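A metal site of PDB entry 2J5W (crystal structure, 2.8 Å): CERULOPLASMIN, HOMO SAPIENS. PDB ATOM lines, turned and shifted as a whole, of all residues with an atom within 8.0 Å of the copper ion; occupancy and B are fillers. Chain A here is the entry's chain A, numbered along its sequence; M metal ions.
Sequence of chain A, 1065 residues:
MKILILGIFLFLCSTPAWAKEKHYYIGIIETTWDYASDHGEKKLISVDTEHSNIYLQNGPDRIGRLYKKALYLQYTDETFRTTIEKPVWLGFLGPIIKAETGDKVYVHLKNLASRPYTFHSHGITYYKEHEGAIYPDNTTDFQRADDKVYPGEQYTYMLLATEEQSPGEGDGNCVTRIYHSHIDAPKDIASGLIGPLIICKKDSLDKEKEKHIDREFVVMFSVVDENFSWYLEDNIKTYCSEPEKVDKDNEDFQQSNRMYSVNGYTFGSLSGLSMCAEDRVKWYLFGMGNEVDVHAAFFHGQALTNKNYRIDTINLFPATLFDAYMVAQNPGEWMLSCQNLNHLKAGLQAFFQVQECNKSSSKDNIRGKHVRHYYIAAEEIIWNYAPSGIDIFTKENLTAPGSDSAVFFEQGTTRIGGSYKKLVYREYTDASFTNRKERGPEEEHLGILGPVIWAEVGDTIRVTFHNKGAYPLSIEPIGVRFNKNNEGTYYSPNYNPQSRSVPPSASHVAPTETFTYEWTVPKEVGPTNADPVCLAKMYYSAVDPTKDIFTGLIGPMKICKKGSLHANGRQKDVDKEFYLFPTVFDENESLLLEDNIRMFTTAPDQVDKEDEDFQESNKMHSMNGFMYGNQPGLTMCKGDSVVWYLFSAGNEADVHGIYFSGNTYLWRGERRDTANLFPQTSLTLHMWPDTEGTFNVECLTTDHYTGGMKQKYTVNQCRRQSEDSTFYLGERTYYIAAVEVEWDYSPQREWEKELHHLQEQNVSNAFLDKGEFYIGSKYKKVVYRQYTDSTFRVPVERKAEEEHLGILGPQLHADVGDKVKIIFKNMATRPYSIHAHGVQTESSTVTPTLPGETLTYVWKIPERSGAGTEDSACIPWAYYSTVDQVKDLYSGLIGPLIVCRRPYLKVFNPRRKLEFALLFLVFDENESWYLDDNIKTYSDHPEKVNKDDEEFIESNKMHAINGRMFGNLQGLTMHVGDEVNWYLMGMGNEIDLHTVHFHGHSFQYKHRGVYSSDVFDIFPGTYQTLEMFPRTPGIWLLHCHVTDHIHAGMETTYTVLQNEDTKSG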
ATOM      1  N   PRO A 582      20.367   5.139  15.129  1.00  0.00           N
ATOM      2  CA  PRO A 582      19.493   4.993  16.306  1.00  0.00           C
ATOM      3  C   PRO A 582      18.906   3.585  16.397  1.00  0.00           C
ATOM      4  O   PRO A 582      18.433   3.048  15.385  1.00  0.00           O
ATOM      5  CB  PRO A 582      18.388   6.026  16.054  1.00  0.00           C
ATOM      6  CG  PRO A 582      18.590   6.522  14.590  1.00  0.00           C
ATOM      7  CD  PRO A 582      19.617   5.627  13.957  1.00  0.00           C
ATOM      8  N   THR A 583      18.948   3.002  17.583  1.00  0.00           N
ATOM      9  CA  THR A 583      18.385   1.681  17.785  1.00  0.00           C
ATOM     10  C   THR A 583      18.182   1.424  19.257  1.00  0.00           C
ATOM     11  O   THR A 583      18.866   1.996  20.098  1.00  0.00           O
ATOM     12  CB  THR A 583      19.297   0.537  17.200  1.00  0.00           C
ATOM     13  OG1 THR A 583      18.608  -0.723  17.265  1.00  0.00           O
ATOM     14  CG2 THR A 583      20.609   0.417  17.973  1.00  0.00           C
ATOM     15  N   VAL A 584      17.236   0.552  19.556  1.00  0.00           N
ATOM     16  CA  VAL A 584      17.163  -0.032  20.876  1.00  0.00           C
ATOM     17  C   VAL A 584      18.180  -1.174  20.897  1.00  0.00           C
ATOM     18  O   VAL A 584      17.880  -2.290  20.438  1.00  0.00           O
ATOM     19  CB  VAL A 584      15.734  -0.524  21.200  1.00  0.00           C
ATOM     20  CG1 VAL A 584      15.663  -1.082  22.619  1.00  0.00           C
ATOM     21  CG2 VAL A 584      14.739   0.603  20.998  1.00  0.00           C
ATOM     22  N   HIS A 621      18.231   2.368  24.752  1.00  0.00           N
ATOM     23  CA  HIS A 621      17.688   3.189  23.680  1.00  0.00           C
ATOM     24  C   HIS A 621      18.697   4.285  23.391  1.00  0.00           C
ATOM     25  O   HIS A 621      18.865   5.217  24.187  1.00  0.00           O
ATOM     26  CB  HIS A 621      16.358   3.808  24.094  1.00  0.00           C
ATOM     27  CG  HIS A 621      15.246   2.814  24.272  1.00  0.00           C
ATOM     28  ND1 HIS A 621      15.210   1.917  25.320  1.00  0.00           N
ATOM     29  CD2 HIS A 621      14.115   2.605  23.559  1.00  0.00           C
ATOM     30  CE1 HIS A 621      14.118   1.187  25.226  1.00  0.00           C
ATOM     31  NE2 HIS A 621      13.432   1.580  24.165  1.00  0.00           N
ATOM     32  N   SER A 622      19.359   4.179  22.234  1.00  0.00           N
ATOM     33  CA  SER A 622      20.592   4.913  21.988  1.00  0.00           C
ATOM     34  C   SER A 622      20.785   5.371  20.550  1.00  0.00           C
ATOM     35  O   SER A 622      20.166   4.873  19.613  1.00  0.00           O
ATOM     36  CB  SER A 622      21.775   4.035  22.376  1.00  0.00           C
ATOM     37  OG  SER A 622      21.777   2.850  21.585  1.00  0.00           O
ATOM     38  N   MET A 623      21.695   6.316  20.401  1.00  0.00           N
ATOM     39  CA  MET A 623      22.081   6.866  19.115  1.00  0.00           C
ATOM     40  C   MET A 623      23.585   6.637  19.012  1.00  0.00           C
ATOM     41  O   MET A 623      24.357   7.172  19.815  1.00  0.00           O
ATOM     42  CB  MET A 623      21.738   8.353  19.103  1.00  0.00           C
ATOM     43  CG  MET A 623      20.953   8.827  17.893  1.00  0.00           C
ATOM     44  SD  MET A 623      19.913  10.256  18.306  1.00  0.00           S
ATOM     45  CE  MET A 623      18.759   9.452  19.377  1.00  0.00           C
ATOM     46  N   SER A 648      19.040   2.452  10.497  1.00  0.00           N
ATOM     47  CA  SER A 648      18.706   1.700  11.714  1.00  0.00           C
ATOM     48  C   SER A 648      18.599   0.210  11.455  1.00  0.00           C
ATOM     49  O   SER A 648      18.549  -0.257  10.318  1.00  0.00           O
ATOM     50  CB  SER A 648      17.387   2.207  12.329  1.00  0.00           C
ATOM     51  OG  SER A 648      17.152   1.634  13.619  1.00  0.00           O
ATOM     52  N   ALA A 653      10.059  -2.773  17.530  1.00  0.00           N
ATOM     53  CA  ALA A 653      10.247  -1.651  18.458  1.00  0.00           C
ATOM     54  C   ALA A 653      10.936  -0.471  17.800  1.00  0.00           C
ATOM     55  O   ALA A 653      10.869   0.652  18.306  1.00  0.00           O
ATOM     56  CB  ALA A 653      11.053  -2.079  19.681  1.00  0.00           C
ATOM     57  N   ASP A 654      11.613  -0.716  16.668  1.00  0.00           N
ATOM     58  CA  ASP A 654      12.438   0.301  16.035  1.00  0.00           C
ATOM     59  C   ASP A 654      11.595   1.034  15.005  1.00  0.00           C
ATOM     60  O   ASP A 654      11.714   0.817  13.792  1.00  0.00           O
ATOM     61  CB  ASP A 654      13.728  -0.308  15.448  1.00  0.00           C
ATOM     62  CG  ASP A 654      14.633  -0.926  16.556  1.00  0.00           C
ATOM     63  OD1 ASP A 654      14.336  -2.061  17.032  1.00  0.00           O
ATOM     64  OD2 ASP A 654      15.638  -0.274  16.941  1.00  0.00           O
ATOM     65  N   VAL A 655      10.699   1.853  15.550  1.00  0.00           N
ATOM     66  CA  VAL A 655       9.934   2.850  14.807  1.00  0.00           C
ATOM     67  C   VAL A 655      10.470   4.206  15.261  1.00  0.00           C
ATOM     68  O   VAL A 655      10.166   4.659  16.376  1.00  0.00           O
ATOM     69  CB  VAL A 655       8.432   2.731  15.119  1.00  0.00           C
ATOM     70  CG1 VAL A 655       7.681   3.927  14.549  1.00  0.00           C
ATOM     71  CG2 VAL A 655       7.880   1.408  14.580  1.00  0.00           C
ATOM     72  N   HIS A 656      11.281   4.845  14.422  1.00  0.00           N
ATOM     73  CA  HIS A 656      12.005   6.021  14.852  1.00  0.00           C
ATOM     74  C   HIS A 656      11.535   7.216  14.074  1.00  0.00           C
ATOM     75  O   HIS A 656      11.132   7.078  12.937  1.00  0.00           O
ATOM     76  CB  HIS A 656      13.495   5.847  14.627  1.00  0.00           C
ATOM     77  CG  HIS A 656      14.079   4.665  15.335  1.00  0.00           C
ATOM     78  ND1 HIS A 656      14.233   4.622  16.711  1.00  0.00           N
ATOM     79  CD2 HIS A 656      14.551   3.494  14.869  1.00  0.00           C
ATOM     80  CE1 HIS A 656      14.775   3.472  17.058  1.00  0.00           C
ATOM     81  NE2 HIS A 656      14.978   2.765  15.965  1.00  0.00           N
ATOM     82  N   GLY A 657      11.576   8.372  14.722  1.00  0.00           N
ATOM     83  CA  GLY A 657      11.328   9.650  14.091  1.00  0.00           C
ATOM     84  C   GLY A 657      12.411  10.588  14.620  1.00  0.00           C
ATOM     85  O   GLY A 657      12.314  11.090  15.742  1.00  0.00           O
ATOM     86  N   ILE A 658      13.448  10.798  13.815  1.00  0.00           N
ATOM     87  CA  ILE A 658      14.640  11.484  14.280  1.00  0.00           C
ATOM     88  C   ILE A 658      14.507  12.959  13.968  1.00  0.00           C
ATOM     89  O   ILE A 658      14.680  13.403  12.821  1.00  0.00           O
ATOM     90  CB  ILE A 658      15.885  10.883  13.657  1.00  0.00           C
ATOM     91  CG1 ILE A 658      15.955   9.376  13.989  1.00  0.00           C
ATOM     92  CG2 ILE A 658      17.108  11.639  14.113  1.00  0.00           C
ATOM     93  CD1 ILE A 658      16.212   9.056  15.429  1.00  0.00           C
ATOM     94  N   ALA A 675      12.989  12.398  10.652  1.00  0.00           N
ATOM     95  CA  ALA A 675      13.271  11.322   9.699  1.00  0.00           C
ATOM     96  C   ALA A 675      12.898   9.971  10.282  1.00  0.00           C
ATOM     97  O   ALA A 675      13.470   9.545  11.279  1.00  0.00           O
ATOM     98  CB  ALA A 675      14.745  11.330   9.337  1.00  0.00           C
ATOM     99  N   LEU A 677      12.879   6.026  10.557  1.00  0.00           N
ATOM    100  CA  LEU A 677      13.698   4.844  10.287  1.00  0.00           C
ATOM    101  C   LEU A 677      13.102   3.592  10.916  1.00  0.00           C
ATOM    102  O   LEU A 677      12.626   3.612  12.051  1.00  0.00           O
ATOM    103  CB  LEU A 677      15.110   5.026  10.844  1.00  0.00           C
ATOM    104  CG  LEU A 677      15.935   6.183  10.297  1.00  0.00           C
ATOM    105  CD1 LEU A 677      17.171   6.347  11.156  1.00  0.00           C
ATOM    106  CD2 LEU A 677      16.308   5.925   8.858  1.00  0.00           C
ATOM    107  N   GLU A 698      16.892  14.102  18.219  1.00  0.00           N
ATOM    108  CA  GLU A 698      16.250  13.224  19.173  1.00  0.00           C
ATOM    109  C   GLU A 698      15.203  12.399  18.491  1.00  0.00           C
ATOM    110  O   GLU A 698      14.665  12.829  17.477  1.00  0.00           O
ATOM    111  CB  GLU A 698      15.638  14.054  20.313  1.00  0.00           C
ATOM    112  CG  GLU A 698      14.444  14.896  19.892  1.00  0.00           C
ATOM    113  CD  GLU A 698      14.021  15.908  20.945  1.00  0.00           C
ATOM    114  OE1 GLU A 698      14.886  16.394  21.727  1.00  0.00           O
ATOM    115  OE2 GLU A 698      12.820  16.228  20.982  1.00  0.00           O
ATOM    116  N   CYS A 699      14.951  11.201  19.014  1.00  0.00           N
ATOM    117  CA  CYS A 699      13.845  10.403  18.537  1.00  0.00           C
ATOM    118  C   CYS A 699      12.587  10.868  19.273  1.00  0.00           C
ATOM    119  O   CYS A 699      12.575  10.936  20.504  1.00  0.00           O
ATOM    120  CB  CYS A 699      14.109   8.913  18.783  1.00  0.00           C
ATOM    121  SG  CYS A 699      12.857   7.868  18.026  1.00  0.00           S
ATOM    122  N   LEU A 700      11.561  11.238  18.507  1.00  0.00           N
ATOM    123  CA  LEU A 700      10.276  11.680  19.050  1.00  0.00           C
ATOM    124  C   LEU A 700       9.435  10.517  19.567  1.00  0.00           C
ATOM    125  O   LEU A 700       8.420  10.754  20.224  1.00  0.00           O
ATOM    126  CB  LEU A 700       9.426  12.300  17.959  1.00  0.00           C
ATOM    127  CG  LEU A 700       9.808  13.548  17.219  1.00  0.00           C
ATOM    128  CD1 LEU A 700       8.932  13.613  15.975  1.00  0.00           C
ATOM    129  CD2 LEU A 700       9.630  14.771  18.082  1.00  0.00           C
ATOM    130  N   THR A 701       9.770   9.284  19.178  1.00  0.00           N
ATOM    131  CA  THR A 701       8.985   8.130  19.631  1.00  0.00           C
ATOM    132  C   THR A 701       9.061   8.103  21.158  1.00  0.00           C
ATOM    133  O   THR A 701      10.135   7.954  21.730  1.00  0.00           O
ATOM    134  CB  THR A 701       9.463   6.809  18.991  1.00  0.00           C
ATOM    135  OG1 THR A 701       9.433   6.919  17.563  1.00  0.00           O
ATOM    136  CG2 THR A 701       8.586   5.677  19.402  1.00  0.00           C
ATOM    137  N   THR A 702       7.919   8.289  21.805  1.00  0.00           N
ATOM    138  CA  THR A 702       7.891   8.761  23.187  1.00  0.00           C
ATOM    139  C   THR A 702       8.659   7.856  24.143  1.00  0.00           C
ATOM    140  O   THR A 702       9.407   8.344  25.000  1.00  0.00           O
ATOM    141  CB  THR A 702       6.451   8.973  23.683  1.00  0.00           C
ATOM    142  OG1 THR A 702       5.641   7.850  23.335  1.00  0.00           O
ATOM    143  CG2 THR A 702       5.855  10.203  23.038  1.00  0.00           C
ATOM    144  N   ASP A 703       8.509   6.538  23.986  1.00  0.00           N
ATOM    145  CA  ASP A 703       9.291   5.604  24.795  1.00  0.00           C
ATOM    146  C   ASP A 703      10.789   5.740  24.534  1.00  0.00           C
ATOM    147  O   ASP A 703      11.566   5.689  25.471  1.00  0.00           O
ATOM    148  CB  ASP A 703       8.850   4.140  24.607  1.00  0.00           C
ATOM    149  CG  ASP A 703       7.660   3.763  25.538  1.00  0.00           C
ATOM    150  OD1 ASP A 703       7.468   4.413  26.603  1.00  0.00           O
ATOM    151  OD2 ASP A 703       6.934   2.793  25.204  1.00  0.00           O
ATOM    152  N   HIS A 704      11.183   5.952  23.287  1.00  0.00           N
ATOM    153  CA  HIS A 704      12.596   6.083  22.959  1.00  0.00           C
ATOM    154  C   HIS A 704      13.159   7.359  23.594  1.00  0.00           C
ATOM    155  O   HIS A 704      14.216   7.337  24.258  1.00  0.00           O
ATOM    156  CB  HIS A 704      12.808   6.088  21.450  1.00  0.00           C
ATOM    157  CG  HIS A 704      12.317   4.854  20.776  1.00  0.00           C
ATOM    158  ND1 HIS A 704      12.570   4.577  19.450  1.00  0.00           N
ATOM    159  CD2 HIS A 704      11.609   3.790  21.251  1.00  0.00           C
ATOM    160  CE1 HIS A 704      12.013   3.419  19.128  1.00  0.00           C
ATOM    161  NE2 HIS A 704      11.433   2.912  20.211  1.00  0.00           N
ATOM    162  N   TYR A 705      12.431   8.463  23.434  1.00  0.00           N
ATOM    163  CA  TYR A 705      12.840   9.711  24.062  1.00  0.00           C
ATOM    164  C   TYR A 705      13.065   9.520  25.574  1.00  0.00           C
ATOM    165  O   TYR A 705      14.137   9.801  26.093  1.00  0.00           O
ATOM    166  CB  TYR A 705      11.820  10.816  23.817  1.00  0.00           C
ATOM    167  CG  TYR A 705      12.308  12.152  24.308  1.00  0.00           C
ATOM    168  CD1 TYR A 705      13.115  12.957  23.513  1.00  0.00           C
ATOM    169  CD2 TYR A 705      11.996  12.586  25.583  1.00  0.00           C
ATOM    170  CE1 TYR A 705      13.577  14.187  23.977  1.00  0.00           C
ATOM    171  CE2 TYR A 705      12.439  13.807  26.039  1.00  0.00           C
ATOM    172  CZ  TYR A 705      13.228  14.599  25.249  1.00  0.00           C
ATOM    173  OH  TYR A 705      13.664  15.792  25.741  1.00  0.00           O
ATOM    174  N   MET A 709      16.973   8.113  23.934  1.00  0.00           N
ATOM    175  CA  MET A 709      17.355   8.270  22.518  1.00  0.00           C
ATOM    176  C   MET A 709      17.307   9.754  22.145  1.00  0.00           C
ATOM    177  O   MET A 709      16.485  10.176  21.329  1.00  0.00           O
ATOM    178  CB  MET A 709      16.436   7.430  21.619  1.00  0.00           C
ATOM    179  CG  MET A 709      17.031   7.084  20.258  1.00  0.00           C
ATOM    180  SD  MET A 709      16.029   5.978  19.208  1.00  0.00           S
ATOM    181  CE  MET A 709      16.305   4.394  20.008  1.00  0.00           C
ATOM    182  N   GLU A 990       5.993   3.768  19.951  1.00  0.00           N
ATOM    183  CA  GLU A 990       6.436   2.687  19.060  1.00  0.00           C
ATOM    184  C   GLU A 990       5.302   2.054  18.282  1.00  0.00           C
ATOM    185  O   GLU A 990       5.491   1.591  17.177  1.00  0.00           O
ATOM    186  CB  GLU A 990       7.088   1.568  19.872  1.00  0.00           C
ATOM    187  CG  GLU A 990       8.339   1.980  20.597  1.00  0.00           C
ATOM    188  CD  GLU A 990       8.976   0.855  21.379  1.00  0.00           C
ATOM    189  OE1 GLU A 990       8.297  -0.168  21.585  1.00  0.00           O
ATOM    190  OE2 GLU A 990      10.150   0.997  21.785  1.00  0.00           O
HETATM  191 CU    CU M   1      13.349   5.870  18.128  1.00  0.00          CU
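O of His 621 lies within hydrogen-bond range of N of Met 709, at 3.5 Å.
A ring nitrogen (ND1) of His 656 lies close to the side-chain sulfur (SD) of Met 709, at 3.4 Å.
The backbone carbonyl oxygen (O) of Val 655 lies within hydrogen-bond range of the side-chain hydroxyl (OG1) of Thr 701.
OD2 of Asp 654 lies within hydrogen-bond range of NE2 of His 656.
A ring nitrogen (NE2) of His 704 lies within hydrogen-bond range of the backbone carbonyl oxygen of Ala 653, 3.0 Å away.
The backbone carbonyl oxygen (O) of Leu 677 lies within hydrogen-bond range of the backbone NH (N) of His 656, 3.0 Å away.
OE2 of Glu 990 lies within hydrogen-bond range of NE2 of His 704 (2.8 Å).
OG1 of Thr 701 lies close to SG of Cys 699 (3.6 Å).
Residues that only touch the copper ion: Val 655.
The copper ion is bound by a ring nitrogen (ND1) of His 704 (2.0 Å), the side-chain sulfur of Cys 699 (2.1 Å) and a ring nitrogen (ND1) of His 656 (2.1 Å).
Slightly farther from the copper ion lies SD of Met 709 (2.9 Å).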
